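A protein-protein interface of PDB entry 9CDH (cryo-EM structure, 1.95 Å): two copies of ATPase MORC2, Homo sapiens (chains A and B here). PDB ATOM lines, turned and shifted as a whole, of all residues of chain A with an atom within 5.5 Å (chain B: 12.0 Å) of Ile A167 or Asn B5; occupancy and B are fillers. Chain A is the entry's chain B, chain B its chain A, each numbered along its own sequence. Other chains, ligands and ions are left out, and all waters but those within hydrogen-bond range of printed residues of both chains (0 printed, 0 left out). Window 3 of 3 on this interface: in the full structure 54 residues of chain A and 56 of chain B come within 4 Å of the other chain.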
ATOM      1  N   VAL A 162     -16.377 -17.015   5.050  1.00  0.00           N
ATOM      2  CA  VAL A 162     -15.125 -16.431   5.515  1.00  0.00           C
ATOM      3  C   VAL A 162     -15.394 -15.228   6.406  1.00  0.00           C
ATOM      4  O   VAL A 162     -14.658 -14.985   7.367  1.00  0.00           O
ATOM      5  CB  VAL A 162     -14.223 -16.058   4.323  1.00  0.00           C
ATOM      6  CG1 VAL A 162     -13.839 -17.303   3.543  1.00  0.00           C
ATOM      7  CG2 VAL A 162     -14.910 -15.046   3.419  1.00  0.00           C
ATOM      8  N   GLU A 163     -16.438 -14.454   6.107  1.00  0.00           N
ATOM      9  CA  GLU A 163     -16.800 -13.336   6.973  1.00  0.00           C
ATOM     10  C   GLU A 163     -17.159 -13.827   8.370  1.00  0.00           C
ATOM     11  O   GLU A 163     -16.706 -13.265   9.376  1.00  0.00           O
ATOM     12  CB  GLU A 163     -17.961 -12.560   6.345  1.00  0.00           C
ATOM     13  CG  GLU A 163     -18.748 -11.670   7.299  1.00  0.00           C
ATOM     14  CD  GLU A 163     -20.034 -12.324   7.774  1.00  0.00           C
ATOM     15  OE1 GLU A 163     -20.846 -12.733   6.917  1.00  0.00           O
ATOM     16  OE2 GLU A 163     -20.240 -12.428   9.000  1.00  0.00           O
ATOM     17  N   LYS A 164     -17.964 -14.887   8.451  1.00  0.00           N
ATOM     18  CA  LYS A 164     -18.313 -15.442   9.751  1.00  0.00           C
ATOM     19  C   LYS A 164     -17.077 -15.948  10.475  1.00  0.00           C
ATOM     20  O   LYS A 164     -16.918 -15.721  11.677  1.00  0.00           O
ATOM     21  CB  LYS A 164     -19.326 -16.572   9.594  1.00  0.00           C
ATOM     22  CG  LYS A 164     -19.804 -17.160  10.913  1.00  0.00           C
ATOM     23  CD  LYS A 164     -20.521 -18.475  10.702  1.00  0.00           C
ATOM     24  CE  LYS A 164     -20.984 -19.072  12.015  1.00  0.00           C
ATOM     25  NZ  LYS A 164     -21.482 -20.461  11.840  1.00  0.00           N
ATOM     26  N   PHE A 165     -16.192 -16.648   9.762  1.00  0.00           N
ATOM     27  CA  PHE A 165     -14.994 -17.168  10.410  1.00  0.00           C
ATOM     28  C   PHE A 165     -14.122 -16.038  10.935  1.00  0.00           C
ATOM     29  O   PHE A 165     -13.590 -16.120  12.046  1.00  0.00           O
ATOM     30  CB  PHE A 165     -14.199 -18.043   9.446  1.00  0.00           C
ATOM     31  CG  PHE A 165     -12.961 -18.624  10.057  1.00  0.00           C
ATOM     32  CD1 PHE A 165     -13.019 -19.795  10.790  1.00  0.00           C
ATOM     33  CD2 PHE A 165     -11.741 -17.987   9.919  1.00  0.00           C
ATOM     34  CE1 PHE A 165     -11.883 -20.323  11.362  1.00  0.00           C
ATOM     35  CE2 PHE A 165     -10.604 -18.512  10.490  1.00  0.00           C
ATOM     36  CZ  PHE A 165     -10.675 -19.680  11.212  1.00  0.00           C
ATOM     37  N   ALA A 166     -13.955 -14.978  10.144  1.00  0.00           N
ATOM     38  CA  ALA A 166     -13.149 -13.848  10.585  1.00  0.00           C
ATOM     39  C   ALA A 166     -13.756 -13.191  11.814  1.00  0.00           C
ATOM     40  O   ALA A 166     -13.038 -12.859  12.761  1.00  0.00           O
ATOM     41  CB  ALA A 166     -13.003 -12.835   9.451  1.00  0.00           C
ATOM     42  N   ILE A 167     -15.077 -13.003  11.827  1.00  0.00           N
ATOM     43  CA  ILE A 167     -15.717 -12.400  12.993  1.00  0.00           C
ATOM     44  C   ILE A 167     -15.532 -13.289  14.217  1.00  0.00           C
ATOM     45  O   ILE A 167     -15.218 -12.810  15.312  1.00  0.00           O
ATOM     46  CB  ILE A 167     -17.203 -12.125  12.711  1.00  0.00           C
ATOM     47  CG1 ILE A 167     -17.346 -10.914  11.796  1.00  0.00           C
ATOM     48  CG2 ILE A 167     -17.954 -11.877  14.008  1.00  0.00           C
ATOM     49  CD1 ILE A 167     -18.588 -10.942  10.959  1.00  0.00           C
ATOM     50  N   GLU A 168     -15.727 -14.597  14.049  1.00  0.00           N
ATOM     51  CA  GLU A 168     -15.583 -15.522  15.166  1.00  0.00           C
ATOM     52  C   GLU A 168     -14.168 -15.493  15.726  1.00  0.00           C
ATOM     53  O   GLU A 168     -13.963 -15.425  16.943  1.00  0.00           O
ATOM     54  CB  GLU A 168     -15.946 -16.936  14.713  1.00  0.00           C
ATOM     55  CG  GLU A 168     -17.402 -17.121  14.344  1.00  0.00           C
ATOM     56  CD  GLU A 168     -17.671 -18.471  13.714  1.00  0.00           C
ATOM     57  OE1 GLU A 168     -17.109 -18.748  12.635  1.00  0.00           O
ATOM     58  OE2 GLU A 168     -18.443 -19.257  14.302  1.00  0.00           O
ATOM     59  N   THR A 169     -13.173 -15.539  14.840  1.00  0.00           N
ATOM     60  CA  THR A 169     -11.789 -15.566  15.291  1.00  0.00           C
ATOM     61  C   THR A 169     -11.394 -14.243  15.930  1.00  0.00           C
ATOM     62  O   THR A 169     -10.647 -14.224  16.912  1.00  0.00           O
ATOM     63  CB  THR A 169     -10.858 -15.900  14.128  1.00  0.00           C
ATOM     64  OG1 THR A 169     -11.201 -15.107  12.987  1.00  0.00           O
ATOM     65  CG2 THR A 169     -10.967 -17.370  13.772  1.00  0.00           C
ATOM     66  N   GLU A 170     -11.878 -13.124  15.388  1.00  0.00           N
ATOM     67  CA  GLU A 170     -11.575 -11.840  16.003  1.00  0.00           C
ATOM     68  C   GLU A 170     -12.226 -11.716  17.370  1.00  0.00           C
ATOM     69  O   GLU A 170     -11.622 -11.166  18.293  1.00  0.00           O
ATOM     70  CB  GLU A 170     -12.019 -10.699  15.090  1.00  0.00           C
ATOM     71  CG  GLU A 170     -11.060 -10.422  13.940  1.00  0.00           C
ATOM     72  CD  GLU A 170      -9.637 -10.164  14.402  1.00  0.00           C
ATOM     73  OE1 GLU A 170      -9.457  -9.688  15.543  1.00  0.00           O
ATOM     74  OE2 GLU A 170      -8.699 -10.444  13.629  1.00  0.00           O
ATOM     75  N   LEU A 171     -13.445 -12.235  17.528  1.00  0.00           N
ATOM     76  CA  LEU A 171     -14.062 -12.255  18.848  1.00  0.00           C
ATOM     77  C   LEU A 171     -13.249 -13.103  19.813  1.00  0.00           C
ATOM     78  O   LEU A 171     -13.069 -12.731  20.977  1.00  0.00           O
ATOM     79  CB  LEU A 171     -15.493 -12.777  18.750  1.00  0.00           C
ATOM     80  CG  LEU A 171     -16.528 -11.775  18.244  1.00  0.00           C
ATOM     81  CD1 LEU A 171     -17.840 -12.479  17.968  1.00  0.00           C
ATOM     82  CD2 LEU A 171     -16.724 -10.648  19.245  1.00  0.00           C
ATOM     83  N   ILE A 172     -12.753 -14.250  19.346  1.00  0.00           N
ATOM     84  CA  ILE A 172     -11.916 -15.088  20.201  1.00  0.00           C
ATOM     85  C   ILE A 172     -10.657 -14.337  20.612  1.00  0.00           C
ATOM     86  O   ILE A 172     -10.289 -14.312  21.790  1.00  0.00           O
ATOM     87  CB  ILE A 172     -11.581 -16.410  19.486  1.00  0.00           C
ATOM     88  CG1 ILE A 172     -12.826 -17.292  19.401  1.00  0.00           C
ATOM     89  CG2 ILE A 172     -10.467 -17.147  20.216  1.00  0.00           C
ATOM     90  CD1 ILE A 172     -12.738 -18.359  18.351  1.00  0.00           C
ATOM     91  N   ASN B   5     -21.311  -6.315  13.416  1.00  0.00           N
ATOM     92  CA  ASN B   5     -22.501  -7.083  13.068  1.00  0.00           C
ATOM     93  C   ASN B   5     -22.248  -8.576  13.242  1.00  0.00           C
ATOM     94  O   ASN B   5     -21.309  -9.127  12.668  1.00  0.00           O
ATOM     95  CB  ASN B   5     -22.931  -6.782  11.633  1.00  0.00           C
ATOM     96  CG  ASN B   5     -24.205  -7.502  11.244  1.00  0.00           C
ATOM     97  OD1 ASN B   5     -24.185  -8.435  10.443  1.00  0.00           O
ATOM     98  ND2 ASN B   5     -25.324  -7.075  11.817  1.00  0.00           N
ATOM     99  N   TYR B   6     -23.099  -9.226  14.036  1.00  0.00           N
ATOM    100  CA  TYR B   6     -22.939 -10.634  14.377  1.00  0.00           C
ATOM    101  C   TYR B   6     -24.124 -11.473  13.915  1.00  0.00           C
ATOM    102  O   TYR B   6     -24.430 -12.496  14.531  1.00  0.00           O
ATOM    103  CB  TYR B   6     -22.743 -10.785  15.885  1.00  0.00           C
ATOM    104  CG  TYR B   6     -21.629  -9.925  16.422  1.00  0.00           C
ATOM    105  CD1 TYR B   6     -20.352 -10.006  15.891  1.00  0.00           C
ATOM    106  CD2 TYR B   6     -21.859  -9.017  17.443  1.00  0.00           C
ATOM    107  CE1 TYR B   6     -19.333  -9.219  16.370  1.00  0.00           C
ATOM    108  CE2 TYR B   6     -20.846  -8.225  17.927  1.00  0.00           C
ATOM    109  CZ  TYR B   6     -19.583  -8.330  17.387  1.00  0.00           C
ATOM    110  OH  TYR B   6     -18.563  -7.543  17.861  1.00  0.00           O
ATOM    111  N   SER B   7     -24.795 -11.059  12.839  1.00  0.00           N
ATOM    112  CA  SER B   7     -25.976 -11.779  12.379  1.00  0.00           C
ATOM    113  C   SER B   7     -25.632 -13.201  11.957  1.00  0.00           C
ATOM    114  O   SER B   7     -26.394 -14.138  12.220  1.00  0.00           O
ATOM    115  CB  SER B   7     -26.627 -11.023  11.222  1.00  0.00           C
ATOM    116  OG  SER B   7     -25.651 -10.585  10.294  1.00  0.00           O
ATOM    117  N   SER B   8     -24.489 -13.383  11.297  1.00  0.00           N
ATOM    118  CA  SER B   8     -24.124 -14.690  10.767  1.00  0.00           C
ATOM    119  C   SER B   8     -23.668 -15.668  11.841  1.00  0.00           C
ATOM    120  O   SER B   8     -23.630 -16.873  11.574  1.00  0.00           O
ATOM    121  CB  SER B   8     -23.018 -14.536   9.722  1.00  0.00           C
ATOM    122  OG  SER B   8     -21.826 -14.049  10.312  1.00  0.00           O
ATOM    123  N   LEU B   9     -23.327 -15.195  13.033  1.00  0.00           N
ATOM    124  CA  LEU B   9     -22.761 -16.073  14.043  1.00  0.00           C
ATOM    125  C   LEU B   9     -23.832 -16.967  14.656  1.00  0.00           C
ATOM    126  O   LEU B   9     -25.020 -16.639  14.681  1.00  0.00           O
ATOM    127  CB  LEU B   9     -22.070 -15.261  15.134  1.00  0.00           C
ATOM    128  CG  LEU B   9     -20.576 -15.042  14.906  1.00  0.00           C
ATOM    129  CD1 LEU B   9     -20.334 -14.218  13.656  1.00  0.00           C
ATOM    130  CD2 LEU B   9     -19.959 -14.374  16.114  1.00  0.00           C
ATOM    131  N   ASN B  10     -23.388 -18.115  15.158  1.00  0.00           N
ATOM    132  CA  ASN B  10     -24.298 -19.076  15.761  1.00  0.00           C
ATOM    133  C   ASN B  10     -24.918 -18.501  17.025  1.00  0.00           C
ATOM    134  O   ASN B  10     -24.277 -17.743  17.758  1.00  0.00           O
ATOM    135  CB  ASN B  10     -23.562 -20.371  16.090  1.00  0.00           C
ATOM    136  CG  ASN B  10     -23.051 -21.079  14.857  1.00  0.00           C
ATOM    137  OD1 ASN B  10     -22.103 -20.631  14.219  1.00  0.00           O
ATOM    138  ND2 ASN B  10     -23.680 -22.195  14.516  1.00  0.00           N
ATOM    139  N   ARG B  11     -26.169 -18.865  17.276  1.00  0.00           N
ATOM    140  CA  ARG B  11     -26.860 -18.529  18.509  1.00  0.00           C
ATOM    141  C   ARG B  11     -27.156 -19.807  19.275  1.00  0.00           C
ATOM    142  O   ARG B  11     -27.502 -20.829  18.678  1.00  0.00           O
ATOM    143  CB  ARG B  11     -28.170 -17.786  18.233  1.00  0.00           C
ATOM    144  CG  ARG B  11     -28.062 -16.280  18.307  1.00  0.00           C
ATOM    145  CD  ARG B  11     -27.368 -15.722  17.087  1.00  0.00           C
ATOM    146  NE  ARG B  11     -27.508 -14.274  17.003  1.00  0.00           N
ATOM    147  CZ  ARG B  11     -26.840 -13.507  16.154  1.00  0.00           C
ATOM    148  NH1 ARG B  11     -25.987 -14.021  15.285  1.00  0.00           N
ATOM    149  NH2 ARG B  11     -27.036 -12.194  16.177  1.00  0.00           N
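Glu A163 touches just one residue of chain B: Ser B8 (2.6 Å).
Glu A168 touches just these residues of chain B: Leu B9 (3.8 Å) and Asn B10 (3.9 Å).
No residue of chain B comes within 4 Å of Thr A169.
Glu A170 touches none of the printed residues of chain B.
Leu A171 touches just these residues of chain B: Tyr B6 (3.9 Å) and Leu B9 (3.4 Å).
Printed residues of chain A within 4 Å of Tyr B6: Ile A167 (3.6 Å) and Leu A171 (3.9 Å).
Of the printed residues of chain B, Lys A164 touches Ser B8 (3.5 Å) and Asn B10 (2.5 Å).
Of the printed residues of chain A, Leu B9 touches Ile A167, Glu A168 and Leu A171.
Phe A165 touches none of the printed residues of chain B.
Val A162 touches none of the printed residues of chain B.
The nearest residue of chain A that does not touch Asn B5 is Glu A163 (5.0 Å).
The nearest printed residue of chain A that does not touch Ser B8 is Ile A167 (4.5 Å).
The guanidinium group of Arg B11 sits close to the backbone carbonyl oxygen of Tyr B6, 3.1 Å away.
The side-chain hydroxyl (OG) of Ser B7 sits at hydrogen-bond distance from the side-chain amide oxygen (OD1) of Asn B5, at 2.6 Å.
The guanidinium group (NH1) of Arg B11 lies within hydrogen-bond range of the backbone carbonyl oxygen (O) of Leu B9, 2.9 Å away.
The side-chain amide oxygen (OD1) of Asn B10 lies within hydrogen-bond range of the side-chain amino group (NZ) of Lys A164, at 2.5 Å.
The side-chain carboxylate (OE2) of Glu A163 sits at hydrogen-bond distance from the side-chain hydroxyl (OG) of Ser B8, 2.6 Å away.
O of Ser B8 touches CE of Lys A164 (3.5 Å).
Asn B5 touches Ile A167 (O to CD1, 3.7 Å).
CD1 of Tyr B6 touches CG2 of Ile A167 (3.6 Å).
Ile A167 touches Leu B9 (CG2 to CD1, 3.4 Å).
Leu B9 touches Glu A168.
Glu A168 touches Asn B10 (OE2 to OD1, 3.9 Å).
Leu A171 touches Tyr B6 (CD2 to OH, 3.9 Å).
Leu A171 touches Leu B9 (CD1 to CD2, 3.4 Å).
Hydrophobic or aromatic side chains of chain A within 4 Å of the printed part of chain B: Ile A167 and Leu A171.
Of the 7 printed residues of chain B, 5 touch a printed residue of chain A.
Printed residues of chain B that touch a printed residue of chain A: Asn B5, Tyr B6, Ser B8, Leu B9 and Asn B10.
Hydrophobic or aromatic side chains of chain B within 4 Å of the printed part of chain A: Tyr B6 and Leu B9.
Along chain B the printed residues that touch a printed residue of chain A span positions 5 to 10.
Among the printed residues, 10 pairs touch across the chains.
No position is printed for both chains.
Of the 10 pairs that touch across the chains among the printed residues, none has its exchanged pair printed and touching as well.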
